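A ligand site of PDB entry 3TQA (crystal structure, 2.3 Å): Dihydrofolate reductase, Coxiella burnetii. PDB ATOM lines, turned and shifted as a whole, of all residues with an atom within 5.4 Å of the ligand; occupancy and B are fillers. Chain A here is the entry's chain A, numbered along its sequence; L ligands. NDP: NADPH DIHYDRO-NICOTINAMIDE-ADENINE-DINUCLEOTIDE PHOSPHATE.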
ATOM      1  N   ILE A   6     -21.980   1.317  -5.984  1.00  0.00           N
ATOM      2  CA  ILE A   6     -22.665   2.580  -5.748  1.00  0.00           C
ATOM      3  C   ILE A   6     -21.834   3.440  -4.793  1.00  0.00           C
ATOM      4  O   ILE A   6     -21.460   2.985  -3.710  1.00  0.00           O
ATOM      5  CB  ILE A   6     -24.103   2.365  -5.202  1.00  0.00           C
ATOM      6  CG1 ILE A   6     -24.868   3.694  -5.145  1.00  0.00           C
ATOM      7  CG2 ILE A   6     -24.077   1.717  -3.825  1.00  0.00           C
ATOM      8  CD1 ILE A   6     -26.348   3.535  -4.910  1.00  0.00           C
ATOM      9  N   ALA A   7     -21.559   4.673  -5.213  1.00  0.00           N
ATOM     10  CA  ALA A   7     -20.726   5.572  -4.420  1.00  0.00           C
ATOM     11  C   ALA A   7     -20.952   7.029  -4.805  1.00  0.00           C
ATOM     12  O   ALA A   7     -21.211   7.338  -5.962  1.00  0.00           O
ATOM     13  CB  ALA A   7     -19.254   5.214  -4.605  1.00  0.00           C
ATOM     14  N   ALA A   8     -20.861   7.913  -3.814  1.00  0.00           N
ATOM     15  CA  ALA A   8     -20.895   9.350  -4.033  1.00  0.00           C
ATOM     16  C   ALA A   8     -19.480   9.899  -3.944  1.00  0.00           C
ATOM     17  O   ALA A   8     -18.776   9.649  -2.964  1.00  0.00           O
ATOM     18  CB  ALA A   8     -21.803  10.029  -3.012  1.00  0.00           C
ATOM     19  N   MET A   9     -19.063  10.646  -4.967  1.00  0.00           N
ATOM     20  CA  MET A   9     -17.725  11.222  -5.005  1.00  0.00           C
ATOM     21  C   MET A   9     -17.755  12.645  -5.565  1.00  0.00           C
ATOM     22  O   MET A   9     -18.762  13.087  -6.102  1.00  0.00           O
ATOM     23  CB  MET A   9     -16.799  10.358  -5.851  1.00  0.00           C
ATOM     24  CG  MET A   9     -17.124  10.345  -7.343  1.00  0.00           C
ATOM     25  SD  MET A   9     -16.242   9.050  -8.235  1.00  0.00           S
ATOM     26  CE  MET A   9     -17.130   7.605  -7.656  1.00  0.00           C
ATOM     27  N   ILE A  15     -14.017  10.396  -1.567  1.00  0.00           N
ATOM     28  CA  ILE A  15     -15.202   9.767  -0.962  1.00  0.00           C
ATOM     29  C   ILE A  15     -15.328   9.947   0.555  1.00  0.00           C
ATOM     30  O   ILE A  15     -16.446   9.916   1.080  1.00  0.00           O
ATOM     31  CB  ILE A  15     -15.304   8.254  -1.319  1.00  0.00           C
ATOM     32  CG1 ILE A  15     -14.023   7.502  -0.927  1.00  0.00           C
ATOM     33  CG2 ILE A  15     -15.595   8.077  -2.799  1.00  0.00           C
ATOM     34  CD1 ILE A  15     -14.105   6.005  -1.194  1.00  0.00           C
ATOM     35  N   GLY A  16     -14.212  10.142   1.264  1.00  0.00           N
ATOM     36  CA  GLY A  16     -14.253  10.229   2.732  1.00  0.00           C
ATOM     37  C   GLY A  16     -13.174  11.086   3.385  1.00  0.00           C
ATOM     38  O   GLY A  16     -12.225  11.523   2.728  1.00  0.00           O
ATOM     39  N   ARG A  17     -13.352  11.324   4.688  1.00  0.00           N
ATOM     40  CA  ARG A  17     -12.449  12.153   5.475  1.00  0.00           C
ATOM     41  C   ARG A  17     -12.624  11.838   6.962  1.00  0.00           C
ATOM     42  O   ARG A  17     -13.708  12.069   7.514  1.00  0.00           O
ATOM     43  CB  ARG A  17     -12.732  13.642   5.213  1.00  0.00           C
ATOM     44  CG  ARG A  17     -11.780  14.602   5.917  1.00  0.00           C
ATOM     45  CD  ARG A  17     -12.273  16.034   5.810  1.00  0.00           C
ATOM     46  NE  ARG A  17     -13.465  16.272   6.637  1.00  0.00           N
ATOM     47  CZ  ARG A  17     -13.447  16.554   7.942  1.00  0.00           C
ATOM     48  NH1 ARG A  17     -12.301  16.638   8.618  1.00  0.00           N
ATOM     49  NH2 ARG A  17     -14.599  16.748   8.580  1.00  0.00           N
ATOM     50  N   ASN A  18     -11.573  11.323   7.595  1.00  0.00           N
ATOM     51  CA  ASN A  18     -11.623  10.898   9.005  1.00  0.00           C
ATOM     52  C   ASN A  18     -12.782   9.930   9.276  1.00  0.00           C
ATOM     53  O   ASN A  18     -13.516  10.065  10.258  1.00  0.00           O
ATOM     54  CB  ASN A  18     -11.704  12.111   9.947  1.00  0.00           C
ATOM     55  CG  ASN A  18     -10.454  12.971   9.901  1.00  0.00           C
ATOM     56  OD1 ASN A  18      -9.341  12.471   9.761  1.00  0.00           O
ATOM     57  ND2 ASN A  18     -10.635  14.287  10.028  1.00  0.00           N
ATOM     58  N   ASN A  19     -12.932   8.945   8.388  1.00  0.00           N
ATOM     59  CA  ASN A  19     -14.004   7.939   8.454  1.00  0.00           C
ATOM     60  C   ASN A  19     -15.420   8.537   8.420  1.00  0.00           C
ATOM     61  O   ASN A  19     -16.363   7.950   8.971  1.00  0.00           O
ATOM     62  CB  ASN A  19     -13.824   7.040   9.683  1.00  0.00           C
ATOM     63  CG  ASN A  19     -14.440   5.654   9.494  1.00  0.00           C
ATOM     64  OD1 ASN A  19     -14.254   5.014   8.452  1.00  0.00           O
ATOM     65  ND2 ASN A  19     -15.180   5.196  10.495  1.00  0.00           N
ATOM     66  N   GLU A  20     -15.580   9.686   7.764  1.00  0.00           N
ATOM     67  CA  GLU A  20     -16.878  10.348   7.610  1.00  0.00           C
ATOM     68  C   GLU A  20     -17.037  10.881   6.189  1.00  0.00           C
ATOM     69  O   GLU A  20     -16.095  10.842   5.391  1.00  0.00           O
ATOM     70  CB  GLU A  20     -17.008  11.498   8.607  1.00  0.00           C
ATOM     71  CG  GLU A  20     -16.975  11.077  10.073  1.00  0.00           C
ATOM     72  CD  GLU A  20     -16.967  12.258  11.027  1.00  0.00           C
ATOM     73  OE1 GLU A  20     -17.329  13.375  10.608  1.00  0.00           O
ATOM     74  OE2 GLU A  20     -16.598  12.070  12.201  1.00  0.00           O
ATOM     75  N   LEU A  21     -18.233  11.375   5.867  1.00  0.00           N
ATOM     76  CA  LEU A  21     -18.484  12.037   4.584  1.00  0.00           C
ATOM     77  C   LEU A  21     -18.034  13.490   4.674  1.00  0.00           C
ATOM     78  O   LEU A  21     -18.259  14.147   5.695  1.00  0.00           O
ATOM     79  CB  LEU A  21     -19.966  11.977   4.217  1.00  0.00           C
ATOM     80  CG  LEU A  21     -20.557  10.605   3.891  1.00  0.00           C
ATOM     81  CD1 LEU A  21     -22.068  10.707   3.718  1.00  0.00           C
ATOM     82  CD2 LEU A  21     -19.925  10.019   2.631  1.00  0.00           C
ATOM     83  N   TRP A  23     -19.335  15.890   2.972  1.00  0.00           N
ATOM     84  CA  TRP A  23     -20.475  16.712   2.571  1.00  0.00           C
ATOM     85  C   TRP A  23     -21.789  16.142   3.107  1.00  0.00           C
ATOM     86  O   TRP A  23     -21.803  15.079   3.749  1.00  0.00           O
ATOM     87  CB  TRP A  23     -20.545  16.791   1.041  1.00  0.00           C
ATOM     88  CG  TRP A  23     -20.665  15.443   0.385  1.00  0.00           C
ATOM     89  CD1 TRP A  23     -21.801  14.685   0.262  1.00  0.00           C
ATOM     90  CD2 TRP A  23     -19.610  14.697  -0.234  1.00  0.00           C
ATOM     91  NE1 TRP A  23     -21.519  13.510  -0.393  1.00  0.00           N
ATOM     92  CE2 TRP A  23     -20.182  13.486  -0.711  1.00  0.00           C
ATOM     93  CE3 TRP A  23     -18.248  14.930  -0.437  1.00  0.00           C
ATOM     94  CZ2 TRP A  23     -19.430  12.515  -1.373  1.00  0.00           C
ATOM     95  CZ3 TRP A  23     -17.504  13.964  -1.096  1.00  0.00           C
ATOM     96  CH2 TRP A  23     -18.092  12.771  -1.553  1.00  0.00           C
ATOM     97  N   GLY A  44     -17.364  -2.699   3.709  1.00  0.00           N
ATOM     98  CA  GLY A  44     -16.207  -2.963   4.566  1.00  0.00           C
ATOM     99  C   GLY A  44     -16.558  -2.645   6.008  1.00  0.00           C
ATOM    100  O   GLY A  44     -17.529  -1.939   6.275  1.00  0.00           O
ATOM    101  N   ARG A  45     -15.762  -3.161   6.937  1.00  0.00           N
ATOM    102  CA  ARG A  45     -16.031  -3.012   8.365  1.00  0.00           C
ATOM    103  C   ARG A  45     -16.004  -1.547   8.807  1.00  0.00           C
ATOM    104  O   ARG A  45     -16.829  -1.131   9.634  1.00  0.00           O
ATOM    105  CB  ARG A  45     -15.055  -3.839   9.190  1.00  0.00           C
ATOM    106  CG  ARG A  45     -15.410  -3.981  10.673  1.00  0.00           C
ATOM    107  CD  ARG A  45     -14.737  -2.926  11.543  1.00  0.00           C
ATOM    108  NE  ARG A  45     -13.279  -3.001  11.463  1.00  0.00           N
ATOM    109  CZ  ARG A  45     -12.436  -2.061  11.891  1.00  0.00           C
ATOM    110  NH1 ARG A  45     -12.896  -0.937  12.442  1.00  0.00           N
ATOM    111  NH2 ARG A  45     -11.132  -2.239  11.762  1.00  0.00           N
ATOM    112  N   ARG A  46     -15.063  -0.766   8.270  1.00  0.00           N
ATOM    113  CA  ARG A  46     -14.986   0.664   8.583  1.00  0.00           C
ATOM    114  C   ARG A  46     -16.217   1.423   8.081  1.00  0.00           C
ATOM    115  O   ARG A  46     -16.715   2.316   8.754  1.00  0.00           O
ATOM    116  CB  ARG A  46     -13.724   1.303   7.990  1.00  0.00           C
ATOM    117  CG  ARG A  46     -12.402   0.778   8.561  1.00  0.00           C
ATOM    118  CD  ARG A  46     -11.261   1.771   8.350  1.00  0.00           C
ATOM    119  NE  ARG A  46      -9.948   1.115   8.305  1.00  0.00           N
ATOM    120  CZ  ARG A  46      -9.152   1.029   7.237  1.00  0.00           C
ATOM    121  NH1 ARG A  46      -9.506   1.559   6.057  1.00  0.00           N
ATOM    122  NH2 ARG A  46      -7.985   0.411   7.334  1.00  0.00           N
ATOM    123  N   THR A  47     -16.715   1.047   6.903  1.00  0.00           N
ATOM    124  CA  THR A  47     -17.912   1.678   6.347  1.00  0.00           C
ATOM    125  C   THR A  47     -19.150   1.399   7.198  1.00  0.00           C
ATOM    126  O   THR A  47     -20.018   2.263   7.331  1.00  0.00           O
ATOM    127  CB  THR A  47     -18.159   1.245   4.882  1.00  0.00           C
ATOM    128  OG1 THR A  47     -17.136   1.793   4.042  1.00  0.00           O
ATOM    129  CG2 THR A  47     -19.515   1.740   4.378  1.00  0.00           C
ATOM    130  N   SER A  50     -18.937   3.654  10.179  1.00  0.00           N
ATOM    131  CA  SER A  50     -19.291   5.002   9.726  1.00  0.00           C
ATOM    132  C   SER A  50     -20.792   5.232   9.763  1.00  0.00           C
ATOM    133  O   SER A  50     -21.262   6.303  10.163  1.00  0.00           O
ATOM    134  CB  SER A  50     -18.751   5.242   8.311  1.00  0.00           C
ATOM    135  OG  SER A  50     -19.182   6.483   7.787  1.00  0.00           O
ATOM    136  N   ILE A  63     -17.680  -7.102   5.336  1.00  0.00           N
ATOM    137  CA  ILE A  63     -16.439  -7.821   5.083  1.00  0.00           C
ATOM    138  C   ILE A  63     -15.396  -7.417   6.116  1.00  0.00           C
ATOM    139  O   ILE A  63     -15.160  -6.234   6.334  1.00  0.00           O
ATOM    140  CB  ILE A  63     -15.903  -7.537   3.658  1.00  0.00           C
ATOM    141  CG1 ILE A  63     -16.993  -7.768   2.603  1.00  0.00           C
ATOM    142  CG2 ILE A  63     -14.688  -8.405   3.359  1.00  0.00           C
ATOM    143  CD1 ILE A  63     -17.639  -9.144   2.661  1.00  0.00           C
ATOM    144  N   THR A  64     -14.791  -8.404   6.769  1.00  0.00           N
ATOM    145  CA  THR A  64     -13.776  -8.166   7.798  1.00  0.00           C
ATOM    146  C   THR A  64     -12.830  -9.364   7.881  1.00  0.00           C
ATOM    147  O   THR A  64     -13.167 -10.457   7.444  1.00  0.00           O
ATOM    148  CB  THR A  64     -14.430  -7.956   9.182  1.00  0.00           C
ATOM    149  OG1 THR A  64     -13.421  -7.636  10.151  1.00  0.00           O
ATOM    150  CG2 THR A  64     -15.178  -9.207   9.630  1.00  0.00           C
ATOM    151  N   GLN A  65     -11.652  -9.137   8.451  1.00  0.00           N
ATOM    152  CA  GLN A  65     -10.698 -10.221   8.710  1.00  0.00           C
ATOM    153  C   GLN A  65     -10.725 -10.663  10.185  1.00  0.00           C
ATOM    154  O   GLN A  65     -10.109 -11.663  10.535  1.00  0.00           O
ATOM    155  CB  GLN A  65      -9.293  -9.807   8.307  1.00  0.00           C
ATOM    156  CG  GLN A  65      -9.140  -9.561   6.810  1.00  0.00           C
ATOM    157  CD  GLN A  65      -7.763  -9.029   6.435  1.00  0.00           C
ATOM    158  OE1 GLN A  65      -7.041  -9.650   5.653  1.00  0.00           O
ATOM    159  NE2 GLN A  65      -7.407  -7.868   6.976  1.00  0.00           N
ATOM    160  N   GLN A  66     -11.425  -9.908  11.026  1.00  0.00           N
ATOM    161  CA  GLN A  66     -11.581 -10.258  12.442  1.00  0.00           C
ATOM    162  C   GLN A  66     -12.528 -11.447  12.567  1.00  0.00           C
ATOM    163  O   GLN A  66     -13.720 -11.340  12.263  1.00  0.00           O
ATOM    164  CB  GLN A  66     -12.127  -9.071  13.243  1.00  0.00           C
ATOM    165  CG  GLN A  66     -11.246  -7.836  13.208  1.00  0.00           C
ATOM    166  CD  GLN A  66     -11.797  -6.707  14.066  1.00  0.00           C
ATOM    167  OE1 GLN A  66     -11.973  -6.868  15.275  1.00  0.00           O
ATOM    168  NE2 GLN A  66     -12.063  -5.567  13.438  1.00  0.00           N
ATOM    169  N   LEU A  69     -15.415 -11.367  15.402  1.00  0.00           N
ATOM    170  CA  LEU A  69     -16.226 -10.148  15.377  1.00  0.00           C
ATOM    171  C   LEU A  69     -17.689 -10.457  15.090  1.00  0.00           C
ATOM    172  O   LEU A  69     -18.026 -11.032  14.056  1.00  0.00           O
ATOM    173  CB  LEU A  69     -15.694  -9.163  14.322  1.00  0.00           C
ATOM    174  CG  LEU A  69     -16.262  -7.749  14.385  1.00  0.00           C
ATOM    175  CD1 LEU A  69     -15.819  -7.040  15.658  1.00  0.00           C
ATOM    176  CD2 LEU A  69     -15.862  -6.950  13.149  1.00  0.00           C
ATOM    177  N   TYR A  78     -15.427 -13.264   5.514  1.00  0.00           N
ATOM    178  CA  TYR A  78     -14.012 -12.997   5.736  1.00  0.00           C
ATOM    179  C   TYR A  78     -13.239 -12.625   4.459  1.00  0.00           C
ATOM    180  O   TYR A  78     -12.029 -12.389   4.499  1.00  0.00           O
ATOM    181  CB  TYR A  78     -13.355 -14.171   6.460  1.00  0.00           C
ATOM    182  CG  TYR A  78     -14.084 -14.537   7.738  1.00  0.00           C
ATOM    183  CD1 TYR A  78     -14.293 -13.580   8.735  1.00  0.00           C
ATOM    184  CD2 TYR A  78     -14.571 -15.821   7.965  1.00  0.00           C
ATOM    185  CE1 TYR A  78     -14.966 -13.894   9.914  1.00  0.00           C
ATOM    186  CE2 TYR A  78     -15.242 -16.144   9.134  1.00  0.00           C
ATOM    187  CZ  TYR A  78     -15.431 -15.173  10.103  1.00  0.00           C
ATOM    188  OH  TYR A  78     -16.095 -15.484  11.272  1.00  0.00           O
ATOM    189  N   SER A  79     -13.947 -12.577   3.340  1.00  0.00           N
ATOM    190  CA  SER A  79     -13.418 -12.035   2.088  1.00  0.00           C
ATOM    191  C   SER A  79     -14.567 -11.631   1.182  1.00  0.00           C
ATOM    192  O   SER A  79     -15.718 -12.024   1.411  1.00  0.00           O
ATOM    193  CB  SER A  79     -12.508 -13.046   1.381  1.00  0.00           C
ATOM    194  OG  SER A  79     -13.260 -14.132   0.857  1.00  0.00           O
ATOM    195  N   LEU A  80     -14.270 -10.841   0.152  1.00  0.00           N
ATOM    196  CA  LEU A  80     -15.284 -10.445  -0.830  1.00  0.00           C
ATOM    197  C   LEU A  80     -15.736 -11.651  -1.644  1.00  0.00           C
ATOM    198  O   LEU A  80     -16.928 -11.798  -1.923  1.00  0.00           O
ATOM    199  CB  LEU A  80     -14.737  -9.349  -1.743  1.00  0.00           C
ATOM    200  CG  LEU A  80     -15.676  -8.787  -2.824  1.00  0.00           C
ATOM    201  CD1 LEU A  80     -16.998  -8.315  -2.220  1.00  0.00           C
ATOM    202  CD2 LEU A  80     -14.993  -7.658  -3.569  1.00  0.00           C
ATOM    203  N   ILE A  96     -21.097  -1.029  -1.620  1.00  0.00           N
ATOM    204  CA  ILE A  96     -21.224   0.358  -1.182  1.00  0.00           C
ATOM    205  C   ILE A  96     -19.944   0.965  -0.616  1.00  0.00           C
ATOM    206  O   ILE A  96     -19.955   2.112  -0.193  1.00  0.00           O
ATOM    207  CB  ILE A  96     -22.388   0.538  -0.164  1.00  0.00           C
ATOM    208  CG1 ILE A  96     -22.096  -0.177   1.160  1.00  0.00           C
ATOM    209  CG2 ILE A  96     -23.695   0.032  -0.754  1.00  0.00           C
ATOM    210  CD1 ILE A  96     -23.053   0.195   2.272  1.00  0.00           C
ATOM    211  N   GLY A  97     -18.845   0.209  -0.610  1.00  0.00           N
ATOM    212  CA  GLY A  97     -17.560   0.743  -0.166  1.00  0.00           C
ATOM    213  C   GLY A  97     -16.957  -0.061   0.973  1.00  0.00           C
ATOM    214  O   GLY A  97     -17.507  -1.085   1.363  1.00  0.00           O
ATOM    215  N   GLY A  98     -15.826   0.398   1.529  1.00  0.00           N
ATOM    216  CA  GLY A  98     -15.182   1.661   1.185  1.00  0.00           C
ATOM    217  C   GLY A  98     -14.131   1.548   0.094  1.00  0.00           C
ATOM    218  O   GLY A  98     -14.284   0.777  -0.852  1.00  0.00           O
ATOM    219  N   ALA A  99     -13.063   2.323   0.239  1.00  0.00           N
ATOM    220  CA  ALA A  99     -12.004   2.428  -0.773  1.00  0.00           C
ATOM    221  C   ALA A  99     -11.356   1.083  -1.103  1.00  0.00           C
ATOM    222  O   ALA A  99     -11.148   0.761  -2.276  1.00  0.00           O
ATOM    223  CB  ALA A  99     -10.933   3.423  -0.320  1.00  0.00           C
ATOM    224  N   ARG A 100     -11.042   0.299  -0.070  1.00  0.00           N
ATOM    225  CA  ARG A 100     -10.427  -1.014  -0.255  1.00  0.00           C
ATOM    226  C   ARG A 100     -11.380  -2.010  -0.922  1.00  0.00           C
ATOM    227  O   ARG A 100     -10.967  -2.783  -1.772  1.00  0.00           O
ATOM    228  CB  ARG A 100      -9.937  -1.569   1.086  1.00  0.00           C
ATOM    229  CG  ARG A 100      -9.302  -2.957   0.975  1.00  0.00           C
ATOM    230  CD  ARG A 100      -8.721  -3.419   2.307  1.00  0.00           C
ATOM    231  NE  ARG A 100      -8.469  -4.861   2.314  1.00  0.00           N
ATOM    232  CZ  ARG A 100      -8.071  -5.556   3.378  1.00  0.00           C
ATOM    233  NH1 ARG A 100      -7.865  -4.953   4.546  1.00  0.00           N
ATOM    234  NH2 ARG A 100      -7.874  -6.868   3.277  1.00  0.00           N
ATOM    235  N   ILE A 101     -12.653  -1.980  -0.517  1.00  0.00           N
ATOM    236  CA  ILE A 101     -13.652  -2.865  -1.106  1.00  0.00           C
ATOM    237  C   ILE A 101     -13.927  -2.492  -2.560  1.00  0.00           C
ATOM    238  O   ILE A 101     -14.020  -3.371  -3.416  1.00  0.00           O
ATOM    239  CB  ILE A 101     -14.971  -2.855  -0.302  1.00  0.00           C
ATOM    240  CG1 ILE A 101     -14.758  -3.496   1.078  1.00  0.00           C
ATOM    241  CG2 ILE A 101     -16.061  -3.618  -1.035  1.00  0.00           C
ATOM    242  CD1 ILE A 101     -14.447  -4.982   1.028  1.00  0.00           C
ATOM    243  N   PHE A 102     -14.041  -1.194  -2.842  1.00  0.00           N
ATOM    244  CA  PHE A 102     -14.240  -0.713  -4.208  1.00  0.00           C
ATOM    245  C   PHE A 102     -13.116  -1.155  -5.144  1.00  0.00           C
ATOM    246  O   PHE A 102     -13.372  -1.621  -6.249  1.00  0.00           O
ATOM    247  CB  PHE A 102     -14.358   0.822  -4.262  1.00  0.00           C
ATOM    248  CG  PHE A 102     -15.687   1.362  -3.800  1.00  0.00           C
ATOM    249  CD1 PHE A 102     -16.884   0.789  -4.224  1.00  0.00           C
ATOM    250  CD2 PHE A 102     -15.740   2.487  -2.994  1.00  0.00           C
ATOM    251  CE1 PHE A 102     -18.105   1.313  -3.806  1.00  0.00           C
ATOM    252  CE2 PHE A 102     -16.955   3.016  -2.569  1.00  0.00           C
ATOM    253  CZ  PHE A 102     -18.133   2.421  -2.983  1.00  0.00           C
ATOM    254  N   GLU A 104     -11.064  -3.716  -4.872  1.00  0.00           N
ATOM    255  CA  GLU A 104     -11.129  -5.157  -5.099  1.00  0.00           C
ATOM    256  C   GLU A 104     -12.343  -5.561  -5.945  1.00  0.00           C
ATOM    257  O   GLU A 104     -12.267  -6.509  -6.719  1.00  0.00           O
ATOM    258  CB  GLU A 104     -11.157  -5.903  -3.760  1.00  0.00           C
ATOM    259  CG  GLU A 104     -11.061  -7.425  -3.905  1.00  0.00           C
ATOM    260  CD  GLU A 104     -10.966  -8.157  -2.568  1.00  0.00           C
ATOM    261  OE1 GLU A 104     -11.052  -7.489  -1.516  1.00  0.00           O
ATOM    262  OE2 GLU A 104     -10.816  -9.391  -2.584  1.00  0.00           O
ATOM    263  N   VAL A 125      -9.417   9.568   1.590  1.00  0.00           N
ATOM    264  CA  VAL A 125      -9.729   8.327   0.863  1.00  0.00           C
ATOM    265  C   VAL A 125     -10.497   8.613  -0.426  1.00  0.00           C
ATOM    266  O   VAL A 125     -11.338   9.509  -0.473  1.00  0.00           O
ATOM    267  CB  VAL A 125     -10.546   7.345   1.743  1.00  0.00           C
ATOM    268  CG1 VAL A 125      -9.709   6.894   2.938  1.00  0.00           C
ATOM    269  CG2 VAL A 125     -11.844   7.991   2.214  1.00  0.00           C
HETATM  270  PA  NDP L   1     -13.524   0.268   4.187  1.00  0.00           P
HETATM  271  O1A NDP L   1     -13.015  -0.171   2.841  1.00  0.00           O
HETATM  272  O2A NDP L   1     -14.974   0.644   4.369  1.00  0.00           O
HETATM  273  O5B NDP L   1     -13.221  -0.904   5.235  1.00  0.00           O
HETATM  274  C5B NDP L   1     -11.889  -1.331   5.494  1.00  0.00           C
HETATM  275  C4B NDP L   1     -11.998  -2.553   6.384  1.00  0.00           C
HETATM  276  O4B NDP L   1     -12.857  -3.517   5.761  1.00  0.00           O
HETATM  277  C3B NDP L   1     -10.676  -3.260   6.633  1.00  0.00           C
HETATM  278  O3B NDP L   1      -9.990  -2.724   7.762  1.00  0.00           O
HETATM  279  C2B NDP L   1     -11.134  -4.685   6.834  1.00  0.00           C
HETATM  280  O2B NDP L   1     -11.695  -4.858   8.134  1.00  0.00           O
HETATM  281  C1B NDP L   1     -12.287  -4.822   5.867  1.00  0.00           C
HETATM  282  N9A NDP L   1     -11.875  -5.316   4.525  1.00  0.00           N
HETATM  283  C8A NDP L   1     -11.714  -4.570   3.410  1.00  0.00           C
HETATM  284  N7A NDP L   1     -11.344  -5.343   2.358  1.00  0.00           N
HETATM  285  C5A NDP L   1     -11.272  -6.612   2.796  1.00  0.00           C
HETATM  286  C6A NDP L   1     -10.941  -7.930   2.201  1.00  0.00           C
HETATM  287  N6A NDP L   1     -10.601  -8.053   0.901  1.00  0.00           N
HETATM  288  N1A NDP L   1     -10.987  -9.021   3.010  1.00  0.00           N
HETATM  289  C2A NDP L   1     -11.321  -8.927   4.307  1.00  0.00           C
HETATM  290  N3A NDP L   1     -11.635  -7.753   4.904  1.00  0.00           N
HETATM  291  C4A NDP L   1     -11.632  -6.590   4.223  1.00  0.00           C
HETATM  292  O3  NDP L   1     -12.586   1.451   4.778  1.00  0.00           O
HETATM  293  PN  NDP L   1     -12.205   2.783   3.958  1.00  0.00           P
HETATM  294  O1N NDP L   1     -11.584   2.398   2.640  1.00  0.00           O
HETATM  295  O2N NDP L   1     -11.445   3.679   4.909  1.00  0.00           O
HETATM  296  O5D NDP L   1     -13.639   3.460   3.680  1.00  0.00           O
HETATM  297  C5D NDP L   1     -14.337   4.208   4.674  1.00  0.00           C
HETATM  298  C4D NDP L   1     -14.404   5.666   4.247  1.00  0.00           C
HETATM  299  O4D NDP L   1     -15.005   5.754   2.945  1.00  0.00           O
HETATM  300  C3D NDP L   1     -15.239   6.520   5.180  1.00  0.00           C
HETATM  301  O3D NDP L   1     -14.609   7.788   5.386  1.00  0.00           O
HETATM  302  C2D NDP L   1     -16.563   6.700   4.471  1.00  0.00           C
HETATM  303  O2D NDP L   1     -17.165   7.959   4.768  1.00  0.00           O
HETATM  304  C1D NDP L   1     -16.185   6.576   3.001  1.00  0.00           C
HETATM  305  N1N NDP L   1     -17.261   6.008   2.192  1.00  0.00           N
HETATM  306  C2N NDP L   1     -17.863   6.802   1.283  1.00  0.00           C
HETATM  307  C3N NDP L   1     -18.900   6.351   0.484  1.00  0.00           C
HETATM  308  C7N NDP L   1     -19.551   7.256  -0.524  1.00  0.00           C
HETATM  309  O7N NDP L   1     -20.463   6.831  -1.214  1.00  0.00           O
HETATM  310  N7N NDP L   1     -19.130   8.518  -0.631  1.00  0.00           N
HETATM  311  C4N NDP L   1     -19.339   4.922   0.654  1.00  0.00           C
HETATM  312  C5N NDP L   1     -18.638   4.129   1.651  1.00  0.00           C
HETATM  313  C6N NDP L   1     -17.612   4.723   2.384  1.00  0.00           C
HETATM  314  P2B NDP L   1     -10.878  -5.343   9.429  1.00  0.00           P
HETATM  315  O1X NDP L   1      -9.909  -4.216   9.683  1.00  0.00           O
HETATM  316  O2X NDP L   1     -11.953  -5.472  10.487  1.00  0.00           O
HETATM  317  O3X NDP L   1     -10.255  -6.651   9.009  1.00  0.00           O
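The backbone NH of Thr 47 is in hydrogen-bond range of an oxygen (O2A) of the ligand.
OG1 of Thr 47 is in hydrogen-bond range of O2A of the ligand (2.5 Å).
A nitrogen (N6A) of the ligand sits at hydrogen-bond distance from the side-chain carboxylate (OE1) of Glu 104 (2.5 Å).
The backbone NH (N) of Ala 8 is in hydrogen-bond range of an oxygen (O7N) of the ligand (2.8 Å).
O of Ala 8 sits at hydrogen-bond distance from N7N of the ligand (2.6 Å).
An oxygen (O2X) of the ligand sits at hydrogen-bond distance from the side-chain hydroxyl (OG1) of Thr 64, at 2.6 Å.
N of Ala 99 is in hydrogen-bond range of O1N of the ligand, 2.8 Å away.
The backbone NH (N) of Gln 65 sits at hydrogen-bond distance from an oxygen (O3X) of the ligand (2.9 Å).
An oxygen (O1N) of the ligand is in hydrogen-bond range of the backbone NH (N) of Arg 100, at 3.5 Å.
N7A of the ligand lies within hydrogen-bond range of NE of Arg 100 (2.9 Å).
An oxygen (O2X) of the ligand is in hydrogen-bond range of the side-chain amide nitrogen of Gln 66 (3.0 Å).
The backbone NH of Arg 45 is in hydrogen-bond range of an oxygen (O4B) of the ligand, at 3.2 Å.
An oxygen (O2X) of the ligand is in salt-bridge range of the guanidinium group of Arg 45 (3.0 Å).
An oxygen (O2A) of the ligand is in hydrogen-bond range of the backbone NH of Gly 98, at 3.0 Å.
NH1 of Arg 46 is in salt-bridge range of O2N of the ligand (3.1 Å).
O3D of the ligand sits at hydrogen-bond distance from N of Glu 20 (3.2 Å).
O of Glu 20 is in hydrogen-bond range of O2D of the ligand, 3.1 Å away.
N7N of the ligand sits close to O of Ile 15.
The side-chain hydroxyl (OG1) of Thr 64 lies within hydrogen-bond range of the backbone NH (N) of Gln 66.
The side-chain amide nitrogen (NE2) of Gln 66 sits close to the guanidinium group (NE) of Arg 45 (3.5 Å).
The backbone NH (N) of Arg 45 sits at hydrogen-bond distance from the backbone carbonyl oxygen (O) of Ile 63, at 3.2 Å.
The backbone carbonyl oxygen of Asn 19 lies within hydrogen-bond range of the side-chain hydroxyl of Ser 50 (3.4 Å).
N of Ile 15 is in hydrogen-bond range of O of Val 125 (3.0 Å).
The backbone carbonyl oxygen of Gly 97 is in hydrogen-bond range of the backbone NH of Gly 44 (2.9 Å).
O of Val 125 sits close to N of Gly 16.
NH1 of Arg 17 lies close to ND2 of Asn 18, 3.2 Å away.
Residues that only touch the ligand: Ile 96 (3.0 Å), Asn 19 (3.1 Å), Ile 63 (3.2 Å), Ile 101 (3.4 Å), Ala 7 (3.5 Å), Tyr 78 (3.5 Å), Gly 44 (3.6 Å), Gly 16 (3.6 Å), Leu 21 (3.7 Å), Arg 17 (3.8 Å), Ser 50 (3.9 Å), Val 125 (3.9 Å), Ser 79 (3.98 Å) and Gly 97 (3.99 Å).
Hydrophobic or aromatic side chains within 4 Å of the ligand: Ala 7, Ala 8, Ile 15, Leu 21, Ile 63, Ala 99, Ile 101 and Val 125.
27 residues have an atom within 4 Å of the ligand: Ala 7, Ala 8, Ile 15, Gly 16, Arg 17, Asn 19, Glu 20, Leu 21, Gly 44, Arg 45, Arg 46, Thr 47, Ser 50, Ile 63, Thr 64, Gln 65, Gln 66, Tyr 78, Ser 79, Ile 96, Gly 97, Gly 98, Ala 99, Arg 100, Ile 101, Glu 104 and Val 125.
Along chain A the residues within 4 Å of the ligand span positions 7 to 125.
The nearest printed residue that does not touch the ligand is Trp 23 (4.1 Å).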
